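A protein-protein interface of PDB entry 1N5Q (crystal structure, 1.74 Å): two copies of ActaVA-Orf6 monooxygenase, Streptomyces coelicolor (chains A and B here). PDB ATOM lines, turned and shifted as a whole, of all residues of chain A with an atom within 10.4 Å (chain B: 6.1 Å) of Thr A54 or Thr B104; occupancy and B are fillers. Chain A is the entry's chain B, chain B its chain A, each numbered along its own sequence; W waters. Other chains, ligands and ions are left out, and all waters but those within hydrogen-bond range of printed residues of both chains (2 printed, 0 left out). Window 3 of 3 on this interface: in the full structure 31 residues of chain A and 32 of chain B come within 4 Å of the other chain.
N of Thr B104 lies within hydrogen-bond range of O of Ala A52.
The backbone NH of Arg B106 sits at hydrogen-bond distance from the backbone carbonyl oxygen of Tyr A50 (2.7 Å).
N of Thr A54 sits at hydrogen-bond distance from O of Phe B102 (3.0 Å).
O of Gly B107 sits at hydrogen-bond distance from N of Tyr A50.
ND1 of His A51 sits close to O of Thr A49.
The backbone NH of Ser A53 lies within hydrogen-bond range of the backbone carbonyl oxygen of Ala A58 (2.9 Å).
O of Tyr A62 sits at hydrogen-bond distance from N of Thr A49 (2.9 Å).
The side-chain amide nitrogen (NE2) of Gln A24 sits at hydrogen-bond distance from the backbone carbonyl oxygen (O) of Ser A53 (3.0 Å).
The backbone NH of Val B11 lies within hydrogen-bond range of the backbone carbonyl oxygen of Met B103 (2.9 Å).
The backbone NH (N) of Thr A57 lies within hydrogen-bond range of the side-chain hydroxyl (OG) of Ser A53 (3.3 Å).
Thr A49 touches Gly B107 (C to O, 3.5 Å).
O of Tyr A50 touches C of Pro B105 (3.6 Å).
SD of Met B103 touches CG of His A51, 3.5 Å away.
Pro B105 touches His A51 (CA to CD2, 3.8 Å).
Met B103 touches Ala A52 (CA to O, 3.3 Å).
Arg B106 touches Ala A52 (CG to CB, 3.9 Å).
CA of Ser A53 touches CB of Met B103 (3.8 Å).
Thr A54 touches Met B103.
OG1 of Thr B104 touches CG2 of Thr A54, at 3.9 Å.
SD of Met B103 touches CB of Val A60 (3.8 Å).
Printed residues of chain B within 4 Å of Tyr A50: Pro B105, Arg B106 and Gly B107.
Printed residues of chain B within 4 Å of His A51: Met B103 (3.5 Å), Thr B104 (3.1 Å) and Pro B105 (3.8 Å).
Printed residues of chain B within 4 Å of Ala A52: Met B103 (3.3 Å), Thr B104 (2.9 Å) and Arg B106 (3.9 Å).
Thr B104 touches just these residues of chain A: His A51 (3.1 Å), Ala A52 (2.9 Å) and Thr A54 (3.9 Å).
Pro B105 touches two residues of chain A.
Of the printed residues of chain A, Arg B106 touches Tyr A50 and Ala A52.
Printed residues of chain A within 4 Å of Gly B107: Thr A49 (3.5 Å) and Tyr A50 (2.6 Å).
The nearest residue of chain A that does not touch Thr B104 is Tyr A50 (4.3 Å).
Of the 11 printed residues of chain B, 6 touch a printed residue of chain A.
Printed residues of chain B that touch a printed residue of chain A: Phe B102, Met B103, Thr B104, Pro B105, Arg B106 and Gly B107.
Of the 20 printed residues of chain A, 7 touch a printed residue of chain B.
Among the printed residues, no Asp or Glu carboxylate lies within 4 Å of a Lys or Arg side-chain nitrogen of the other chain.
No position is printed for both chains.
Water W1 lies within hydrogen-bond range of OG1 of Thr B104 (2.8 Å), O of Ala A52 (3.0 Å) and O of Ser A53 (3.5 Å).
Water W2 lies within hydrogen-bond range of the side-chain hydroxyl of Thr A54, the backbone NH of Asp A55 and the backbone carbonyl oxygen of Phe B102.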
ATOM      1  N   VAL A  18      -2.752 -39.839  10.180  1.00  0.00           N
ATOM      2  CA  VAL A  18      -1.946 -39.782   8.957  1.00  0.00           C
ATOM      3  C   VAL A  18      -0.650 -40.590   9.147  1.00  0.00           C
ATOM      4  O   VAL A  18      -0.304 -40.996  10.251  1.00  0.00           O
ATOM      5  CB  VAL A  18      -1.629 -38.401   8.422  1.00  0.00           C
ATOM      6  CG1 VAL A  18      -2.941 -37.658   8.036  1.00  0.00           C
ATOM      7  CG2 VAL A  18      -0.823 -37.480   9.337  1.00  0.00           C
ATOM      8  N   GLY A  20       2.431 -39.540   8.371  1.00  0.00           N
ATOM      9  CA  GLY A  20       3.550 -38.677   8.631  1.00  0.00           C
ATOM     10  C   GLY A  20       3.467 -37.225   8.281  1.00  0.00           C
ATOM     11  O   GLY A  20       2.479 -36.754   7.724  1.00  0.00           O
ATOM     12  N   PRO A  21       4.532 -36.463   8.495  1.00  0.00           N
ATOM     13  CA  PRO A  21       4.547 -35.013   8.289  1.00  0.00           C
ATOM     14  C   PRO A  21       4.274 -34.617   6.853  1.00  0.00           C
ATOM     15  O   PRO A  21       3.499 -33.680   6.603  1.00  0.00           O
ATOM     16  CB  PRO A  21       5.852 -34.535   8.828  1.00  0.00           C
ATOM     17  CG  PRO A  21       6.693 -35.747   9.074  1.00  0.00           C
ATOM     18  CD  PRO A  21       5.759 -36.935   9.203  1.00  0.00           C
ATOM     19  N   GLN A  24       0.603 -34.800   6.716  1.00  0.00           N
ATOM     20  CA  GLN A  24       0.022 -33.703   7.492  1.00  0.00           C
ATOM     21  C   GLN A  24       0.035 -32.401   6.670  1.00  0.00           C
ATOM     22  O   GLN A  24      -0.981 -31.737   6.589  1.00  0.00           O
ATOM     23  CB  GLN A  24       0.752 -33.333   8.778  1.00  0.00           C
ATOM     24  CG  GLN A  24       0.768 -34.353   9.878  1.00  0.00           C
ATOM     25  CD  GLN A  24       1.684 -33.985  11.017  1.00  0.00           C
ATOM     26  OE1 GLN A  24       2.792 -33.526  10.845  1.00  0.00           O
ATOM     27  NE2 GLN A  24       1.154 -34.153  12.279  1.00  0.00           N
ATOM     28  N   HIS A  25       1.196 -32.026   6.116  1.00  0.00           N
ATOM     29  CA  HIS A  25       1.244 -30.823   5.279  1.00  0.00           C
ATOM     30  C   HIS A  25       0.258 -30.899   4.127  1.00  0.00           C
ATOM     31  O   HIS A  25      -0.477 -29.930   3.868  1.00  0.00           O
ATOM     32  CB  HIS A  25       2.669 -30.529   4.798  1.00  0.00           C
ATOM     33  CG  HIS A  25       2.774 -29.262   4.002  1.00  0.00           C
ATOM     34  ND1 HIS A  25       3.115 -28.055   4.569  1.00  0.00           N
ATOM     35  CD2 HIS A  25       2.548 -29.020   2.686  1.00  0.00           C
ATOM     36  CE1 HIS A  25       3.115 -27.125   3.623  1.00  0.00           C
ATOM     37  NE2 HIS A  25       2.761 -27.677   2.466  1.00  0.00           N
ATOM     38  N   VAL A  28      -3.462 -30.388   5.407  1.00  0.00           N
ATOM     39  CA  VAL A  28      -3.694 -29.017   5.827  1.00  0.00           C
ATOM     40  C   VAL A  28      -3.852 -28.163   4.564  1.00  0.00           C
ATOM     41  O   VAL A  28      -4.834 -27.409   4.462  1.00  0.00           O
ATOM     42  CB  VAL A  28      -2.619 -28.471   6.760  1.00  0.00           C
ATOM     43  CG1 VAL A  28      -2.729 -26.984   7.075  1.00  0.00           C
ATOM     44  CG2 VAL A  28      -2.675 -29.238   8.105  1.00  0.00           C
ATOM     45  N   THR A  49      -9.585 -24.258  12.657  1.00  0.00           N
ATOM     46  CA  THR A  49      -8.128 -24.117  12.754  1.00  0.00           C
ATOM     47  C   THR A  49      -7.524 -25.497  12.624  1.00  0.00           C
ATOM     48  O   THR A  49      -7.920 -26.403  13.399  1.00  0.00           O
ATOM     49  CB  THR A  49      -7.728 -23.465  14.088  1.00  0.00           C
ATOM     50  OG1 THR A  49      -8.294 -22.148  14.239  1.00  0.00           O
ATOM     51  CG2 THR A  49      -6.185 -23.348  14.188  1.00  0.00           C
ATOM     52  N   TYR A  50      -6.642 -25.719  11.621  1.00  0.00           N
ATOM     53  CA  TYR A  50      -6.046 -27.052  11.489  1.00  0.00           C
ATOM     54  C   TYR A  50      -4.679 -27.075  12.151  1.00  0.00           C
ATOM     55  O   TYR A  50      -3.881 -26.123  12.013  1.00  0.00           O
ATOM     56  CB  TYR A  50      -5.885 -27.390   9.967  1.00  0.00           C
ATOM     57  CG  TYR A  50      -7.207 -27.771   9.340  1.00  0.00           C
ATOM     58  CD1 TYR A  50      -8.134 -26.807   8.923  1.00  0.00           C
ATOM     59  CD2 TYR A  50      -7.515 -29.104   9.174  1.00  0.00           C
ATOM     60  CE1 TYR A  50      -9.344 -27.223   8.369  1.00  0.00           C
ATOM     61  CE2 TYR A  50      -8.706 -29.524   8.619  1.00  0.00           C
ATOM     62  CZ  TYR A  50      -9.612 -28.565   8.216  1.00  0.00           C
ATOM     63  OH  TYR A  50     -10.817 -28.987   7.694  1.00  0.00           O
ATOM     64  N   HIS A  51      -4.374 -28.166  12.880  1.00  0.00           N
ATOM     65  CA  HIS A  51      -3.148 -28.291  13.605  1.00  0.00           C
ATOM     66  C   HIS A  51      -2.439 -29.597  13.177  1.00  0.00           C
ATOM     67  O   HIS A  51      -3.104 -30.540  12.776  1.00  0.00           O
ATOM     68  CB  HIS A  51      -3.328 -28.468  15.131  1.00  0.00           C
ATOM     69  CG  HIS A  51      -4.278 -27.472  15.759  1.00  0.00           C
ATOM     70  ND1 HIS A  51      -5.625 -27.472  15.481  1.00  0.00           N
ATOM     71  CD2 HIS A  51      -4.058 -26.513  16.675  1.00  0.00           C
ATOM     72  CE1 HIS A  51      -6.222 -26.471  16.189  1.00  0.00           C
ATOM     73  NE2 HIS A  51      -5.280 -25.895  16.910  1.00  0.00           N
ATOM     74  N   ALA A  52      -1.120 -29.581  13.225  1.00  0.00           N
ATOM     75  CA  ALA A  52      -0.401 -30.835  13.014  1.00  0.00           C
ATOM     76  C   ALA A  52       0.088 -31.343  14.377  1.00  0.00           C
ATOM     77  O   ALA A  52       0.760 -30.584  15.105  1.00  0.00           O
ATOM     78  CB  ALA A  52       0.865 -30.513  12.198  1.00  0.00           C
ATOM     79  N   SER A  53      -0.194 -32.627  14.699  1.00  0.00           N
ATOM     80  CA  SER A  53       0.329 -33.112  15.981  1.00  0.00           C
ATOM     81  C   SER A  53       1.866 -33.041  15.893  1.00  0.00           C
ATOM     82  O   SER A  53       2.451 -33.211  14.808  1.00  0.00           O
ATOM     83  CB  SER A  53      -0.119 -34.538  16.301  1.00  0.00           C
ATOM     84  OG  SER A  53       0.460 -35.436  15.277  1.00  0.00           O
ATOM     85  N   THR A  54       2.511 -32.880  17.017  1.00  0.00           N
ATOM     86  CA  THR A  54       3.978 -32.762  17.111  1.00  0.00           C
ATOM     87  C   THR A  54       4.665 -34.054  16.685  1.00  0.00           C
ATOM     88  O   THR A  54       5.834 -33.996  16.224  1.00  0.00           O
ATOM     89  CB  THR A  54       4.413 -32.246  18.499  1.00  0.00           C
ATOM     90  OG1 THR A  54       3.737 -33.031  19.499  1.00  0.00           O
ATOM     91  CG2 THR A  54       3.991 -30.793  18.675  1.00  0.00           C
ATOM     92  N   ASP A  55       4.013 -35.210  16.817  1.00  0.00           N
ATOM     93  CA  ASP A  55       4.647 -36.479  16.414  1.00  0.00           C
ATOM     94  C   ASP A  55       4.472 -36.833  14.948  1.00  0.00           C
ATOM     95  O   ASP A  55       4.909 -37.943  14.573  1.00  0.00           O
ATOM     96  CB  ASP A  55       4.136 -37.641  17.285  1.00  0.00           C
ATOM     97  CG  ASP A  55       2.682 -37.995  17.092  1.00  0.00           C
ATOM     98  OD1 ASP A  55       2.006 -37.491  16.153  1.00  0.00           O
ATOM     99  OD2 ASP A  55       2.194 -38.830  17.904  1.00  0.00           O
ATOM    100  N   GLY A  56       3.871 -35.991  14.135  1.00  0.00           N
ATOM    101  CA  GLY A  56       3.666 -36.212  12.709  1.00  0.00           C
ATOM    102  C   GLY A  56       2.510 -37.149  12.392  1.00  0.00           C
ATOM    103  O   GLY A  56       2.238 -37.313  11.178  1.00  0.00           O
ATOM    104  N   THR A  57       1.783 -37.717  13.326  1.00  0.00           N
ATOM    105  CA  THR A  57       0.776 -38.726  13.021  1.00  0.00           C
ATOM    106  C   THR A  57      -0.698 -38.340  12.920  1.00  0.00           C
ATOM    107  O   THR A  57      -1.566 -39.188  12.617  1.00  0.00           O
ATOM    108  CB  THR A  57       0.810 -39.856  14.096  1.00  0.00           C
ATOM    109  OG1 THR A  57       0.375 -39.338  15.356  1.00  0.00           O
ATOM    110  CG2 THR A  57       2.195 -40.455  14.191  1.00  0.00           C
ATOM    111  N   ALA A  58      -0.990 -37.075  13.152  1.00  0.00           N
ATOM    112  CA  ALA A  58      -2.399 -36.653  13.097  1.00  0.00           C
ATOM    113  C   ALA A  58      -2.540 -35.187  12.740  1.00  0.00           C
ATOM    114  O   ALA A  58      -1.637 -34.369  12.912  1.00  0.00           O
ATOM    115  CB  ALA A  58      -3.056 -36.930  14.475  1.00  0.00           C
ATOM    116  N   VAL A  59      -3.696 -34.855  12.142  1.00  0.00           N
ATOM    117  CA  VAL A  59      -4.066 -33.474  11.844  1.00  0.00           C
ATOM    118  C   VAL A  59      -5.379 -33.320  12.635  1.00  0.00           C
ATOM    119  O   VAL A  59      -6.242 -34.165  12.554  1.00  0.00           O
ATOM    120  CB  VAL A  59      -4.251 -33.135  10.361  1.00  0.00           C
ATOM    121  CG1 VAL A  59      -4.872 -31.735  10.185  1.00  0.00           C
ATOM    122  CG2 VAL A  59      -2.894 -33.140   9.671  1.00  0.00           C
ATOM    123  N   VAL A  60      -5.467 -32.188  13.355  1.00  0.00           N
ATOM    124  CA  VAL A  60      -6.671 -31.972  14.175  1.00  0.00           C
ATOM    125  C   VAL A  60      -7.298 -30.629  13.782  1.00  0.00           C
ATOM    126  O   VAL A  60      -6.609 -29.618  13.770  1.00  0.00           O
ATOM    127  CB  VAL A  60      -6.239 -31.914  15.677  1.00  0.00           C
ATOM    128  CG1 VAL A  60      -7.455 -31.531  16.532  1.00  0.00           C
ATOM    129  CG2 VAL A  60      -5.668 -33.258  16.126  1.00  0.00           C
ATOM    130  N   ASN A  61      -8.607 -30.632  13.516  1.00  0.00           N
ATOM    131  CA  ASN A  61      -9.360 -29.400  13.214  1.00  0.00           C
ATOM    132  C   ASN A  61     -10.222 -29.048  14.450  1.00  0.00           C
ATOM    133  O   ASN A  61     -11.026 -29.883  14.867  1.00  0.00           O
ATOM    134  CB  ASN A  61     -10.258 -29.654  11.998  1.00  0.00           C
ATOM    135  CG  ASN A  61     -11.253 -28.523  11.702  1.00  0.00           C
ATOM    136  OD1 ASN A  61     -11.131 -27.431  12.230  1.00  0.00           O
ATOM    137  ND2 ASN A  61     -12.257 -28.784  10.883  1.00  0.00           N
ATOM    138  N   TYR A  62      -9.994 -27.861  15.011  1.00  0.00           N
ATOM    139  CA  TYR A  62     -10.845 -27.304  16.080  1.00  0.00           C
ATOM    140  C   TYR A  62     -11.757 -26.298  15.391  1.00  0.00           C
ATOM    141  O   TYR A  62     -11.215 -25.350  14.822  1.00  0.00           O
ATOM    142  CB  TYR A  62      -9.967 -26.657  17.145  1.00  0.00           C
ATOM    143  CG  TYR A  62     -10.750 -25.973  18.251  1.00  0.00           C
ATOM    144  CD1 TYR A  62     -11.118 -24.644  18.198  1.00  0.00           C
ATOM    145  CD2 TYR A  62     -11.092 -26.760  19.363  1.00  0.00           C
ATOM    146  CE1 TYR A  62     -11.827 -24.058  19.270  1.00  0.00           C
ATOM    147  CE2 TYR A  62     -11.790 -26.153  20.409  1.00  0.00           C
ATOM    148  CZ  TYR A  62     -12.145 -24.840  20.360  1.00  0.00           C
ATOM    149  OH  TYR A  62     -12.833 -24.302  21.476  1.00  0.00           O
ATOM    150  N   VAL B   8      -0.045 -17.937  19.092  1.00  0.00           N
ATOM    151  CA  VAL B   8      -0.267 -19.314  19.578  1.00  0.00           C
ATOM    152  C   VAL B   8       0.690 -20.283  18.877  1.00  0.00           C
ATOM    153  O   VAL B   8       0.432 -20.712  17.729  1.00  0.00           O
ATOM    154  CB  VAL B   8      -1.689 -19.776  19.278  1.00  0.00           C
ATOM    155  CG1 VAL B   8      -1.925 -21.152  19.900  1.00  0.00           C
ATOM    156  CG2 VAL B   8      -2.720 -18.766  19.779  1.00  0.00           C
ATOM    157  N   GLY B   9       1.741 -20.704  19.534  1.00  0.00           N
ATOM    158  CA  GLY B   9       2.743 -21.565  18.934  1.00  0.00           C
ATOM    159  C   GLY B   9       2.554 -23.030  19.300  1.00  0.00           C
ATOM    160  O   GLY B   9       3.170 -23.892  18.682  1.00  0.00           O
ATOM    161  N   PHE B  10       1.755 -23.301  20.361  1.00  0.00           N
ATOM    162  CA  PHE B  10       1.655 -24.681  20.844  1.00  0.00           C
ATOM    163  C   PHE B  10       0.265 -24.901  21.511  1.00  0.00           C
ATOM    164  O   PHE B  10      -0.262 -24.007  22.132  1.00  0.00           O
ATOM    165  CB  PHE B  10       2.722 -24.963  21.873  1.00  0.00           C
ATOM    166  CG  PHE B  10       2.724 -26.327  22.504  1.00  0.00           C
ATOM    167  CD1 PHE B  10       3.296 -27.384  21.809  1.00  0.00           C
ATOM    168  CD2 PHE B  10       2.172 -26.564  23.754  1.00  0.00           C
ATOM    169  CE1 PHE B  10       3.331 -28.660  22.365  1.00  0.00           C
ATOM    170  CE2 PHE B  10       2.192 -27.831  24.292  1.00  0.00           C
ATOM    171  CZ  PHE B  10       2.777 -28.873  23.620  1.00  0.00           C
ATOM    172  N   VAL B  11      -0.346 -26.019  21.163  1.00  0.00           N
ATOM    173  CA  VAL B  11      -1.669 -26.337  21.729  1.00  0.00           C
ATOM    174  C   VAL B  11      -1.685 -27.724  22.347  1.00  0.00           C
ATOM    175  O   VAL B  11      -1.126 -28.677  21.767  1.00  0.00           O
ATOM    176  CB  VAL B  11      -2.737 -26.277  20.617  1.00  0.00           C
ATOM    177  CG1 VAL B  11      -4.093 -26.877  21.018  1.00  0.00           C
ATOM    178  CG2 VAL B  11      -3.009 -24.821  20.205  1.00  0.00           C
ATOM    179  N   GLU B  68       5.992 -24.389  22.980  1.00  0.00           N
ATOM    180  CA  GLU B  68       6.216 -25.635  23.686  1.00  0.00           C
ATOM    181  C   GLU B  68       7.188 -25.447  24.837  1.00  0.00           C
ATOM    182  O   GLU B  68       7.112 -26.004  25.928  1.00  0.00           O
ATOM    183  CB  GLU B  68       6.750 -26.732  22.733  1.00  0.00           C
ATOM    184  CG  GLU B  68       6.895 -28.058  23.484  1.00  0.00           C
ATOM    185  CD  GLU B  68       7.551 -29.157  22.670  1.00  0.00           C
ATOM    186  OE1 GLU B  68       7.117 -29.310  21.515  1.00  0.00           O
ATOM    187  OE2 GLU B  68       8.462 -29.835  23.207  1.00  0.00           O
ATOM    188  N   PHE B 102      -0.670 -33.239  21.650  1.00  0.00           N
ATOM    189  CA  PHE B 102       0.128 -32.000  21.501  1.00  0.00           C
ATOM    190  C   PHE B 102       0.291 -31.663  20.010  1.00  0.00           C
ATOM    191  O   PHE B 102       0.448 -32.553  19.172  1.00  0.00           O
ATOM    192  CB  PHE B 102       1.495 -32.182  22.139  1.00  0.00           C
ATOM    193  CG  PHE B 102       1.380 -32.587  23.584  1.00  0.00           C
ATOM    194  CD1 PHE B 102       0.634 -31.831  24.471  1.00  0.00           C
ATOM    195  CD2 PHE B 102       1.980 -33.777  24.026  1.00  0.00           C
ATOM    196  CE1 PHE B 102       0.523 -32.214  25.821  1.00  0.00           C
ATOM    197  CE2 PHE B 102       1.881 -34.172  25.354  1.00  0.00           C
ATOM    198  CZ  PHE B 102       1.153 -33.395  26.250  1.00  0.00           C
ATOM    199  N   MET B 103       0.126 -30.367  19.729  1.00  0.00           N
ATOM    200  CA  MET B 103       0.000 -30.043  18.274  1.00  0.00           C
ATOM    201  C   MET B 103       0.319 -28.582  18.033  1.00  0.00           C
ATOM    202  O   MET B 103       0.424 -27.817  18.990  1.00  0.00           O
ATOM    203  CB  MET B 103      -1.449 -30.344  17.781  1.00  0.00           C
ATOM    204  CG  MET B 103      -2.504 -29.453  18.523  1.00  0.00           C
ATOM    205  SD  MET B 103      -4.213 -29.997  18.187  1.00  0.00           S
ATOM    206  CE  MET B 103      -4.211 -31.527  19.164  1.00  0.00           C
ATOM    207  N   THR B 104       0.534 -28.215  16.771  1.00  0.00           N
ATOM    208  CA  THR B 104       0.893 -26.863  16.359  1.00  0.00           C
ATOM    209  C   THR B 104      -0.117 -26.342  15.362  1.00  0.00           C
ATOM    210  O   THR B 104      -0.401 -26.998  14.360  1.00  0.00           O
ATOM    211  CB  THR B 104       2.265 -26.997  15.563  1.00  0.00           C
ATOM    212  OG1 THR B 104       3.192 -27.673  16.431  1.00  0.00           O
ATOM    213  CG2 THR B 104       2.733 -25.606  15.235  1.00  0.00           C
ATOM    214  N   PRO B 105      -0.675 -25.147  15.469  1.00  0.00           N
ATOM    215  CA  PRO B 105      -1.618 -24.599  14.536  1.00  0.00           C
ATOM    216  C   PRO B 105      -0.922 -24.431  13.176  1.00  0.00           C
ATOM    217  O   PRO B 105       0.194 -23.887  13.197  1.00  0.00           O
ATOM    218  CB  PRO B 105      -2.006 -23.249  15.145  1.00  0.00           C
ATOM    219  CG  PRO B 105      -1.724 -23.424  16.597  1.00  0.00           C
ATOM    220  CD  PRO B 105      -0.433 -24.233  16.632  1.00  0.00           C
ATOM    221  N   ARG B 106      -1.523 -24.904  12.126  1.00  0.00           N
ATOM    222  CA  ARG B 106      -0.841 -24.817  10.820  1.00  0.00           C
ATOM    223  C   ARG B 106      -1.665 -24.153   9.746  1.00  0.00           C
ATOM    224  O   ARG B 106      -1.036 -23.704   8.753  1.00  0.00           O
ATOM    225  CB  ARG B 106      -0.359 -26.200  10.381  1.00  0.00           C
ATOM    226  CG  ARG B 106       0.822 -26.769  11.142  1.00  0.00           C
ATOM    227  CD  ARG B 106       2.085 -25.925  11.146  1.00  0.00           C
ATOM    228  NE  ARG B 106       3.196 -26.644  11.792  1.00  0.00           N
ATOM    229  CZ  ARG B 106       4.335 -26.161  12.248  1.00  0.00           C
ATOM    230  NH1 ARG B 106       4.645 -24.871  12.177  1.00  0.00           N
ATOM    231  NH2 ARG B 106       5.272 -26.938  12.811  1.00  0.00           N
ATOM    232  N   GLY B 107      -2.968 -24.030   9.869  1.00  0.00           N
ATOM    233  CA  GLY B 107      -3.786 -23.349   8.851  1.00  0.00           C
ATOM    234  C   GLY B 107      -5.142 -22.979   9.449  1.00  0.00           C
ATOM    235  O   GLY B 107      -5.583 -23.647  10.399  1.00  0.00           O
HETATM  236  O   HOH W   1       3.677 -29.939  14.929  1.00  0.00           O
HETATM  237  O   HOH W   2       2.211 -35.398  19.120  1.00  0.00           O
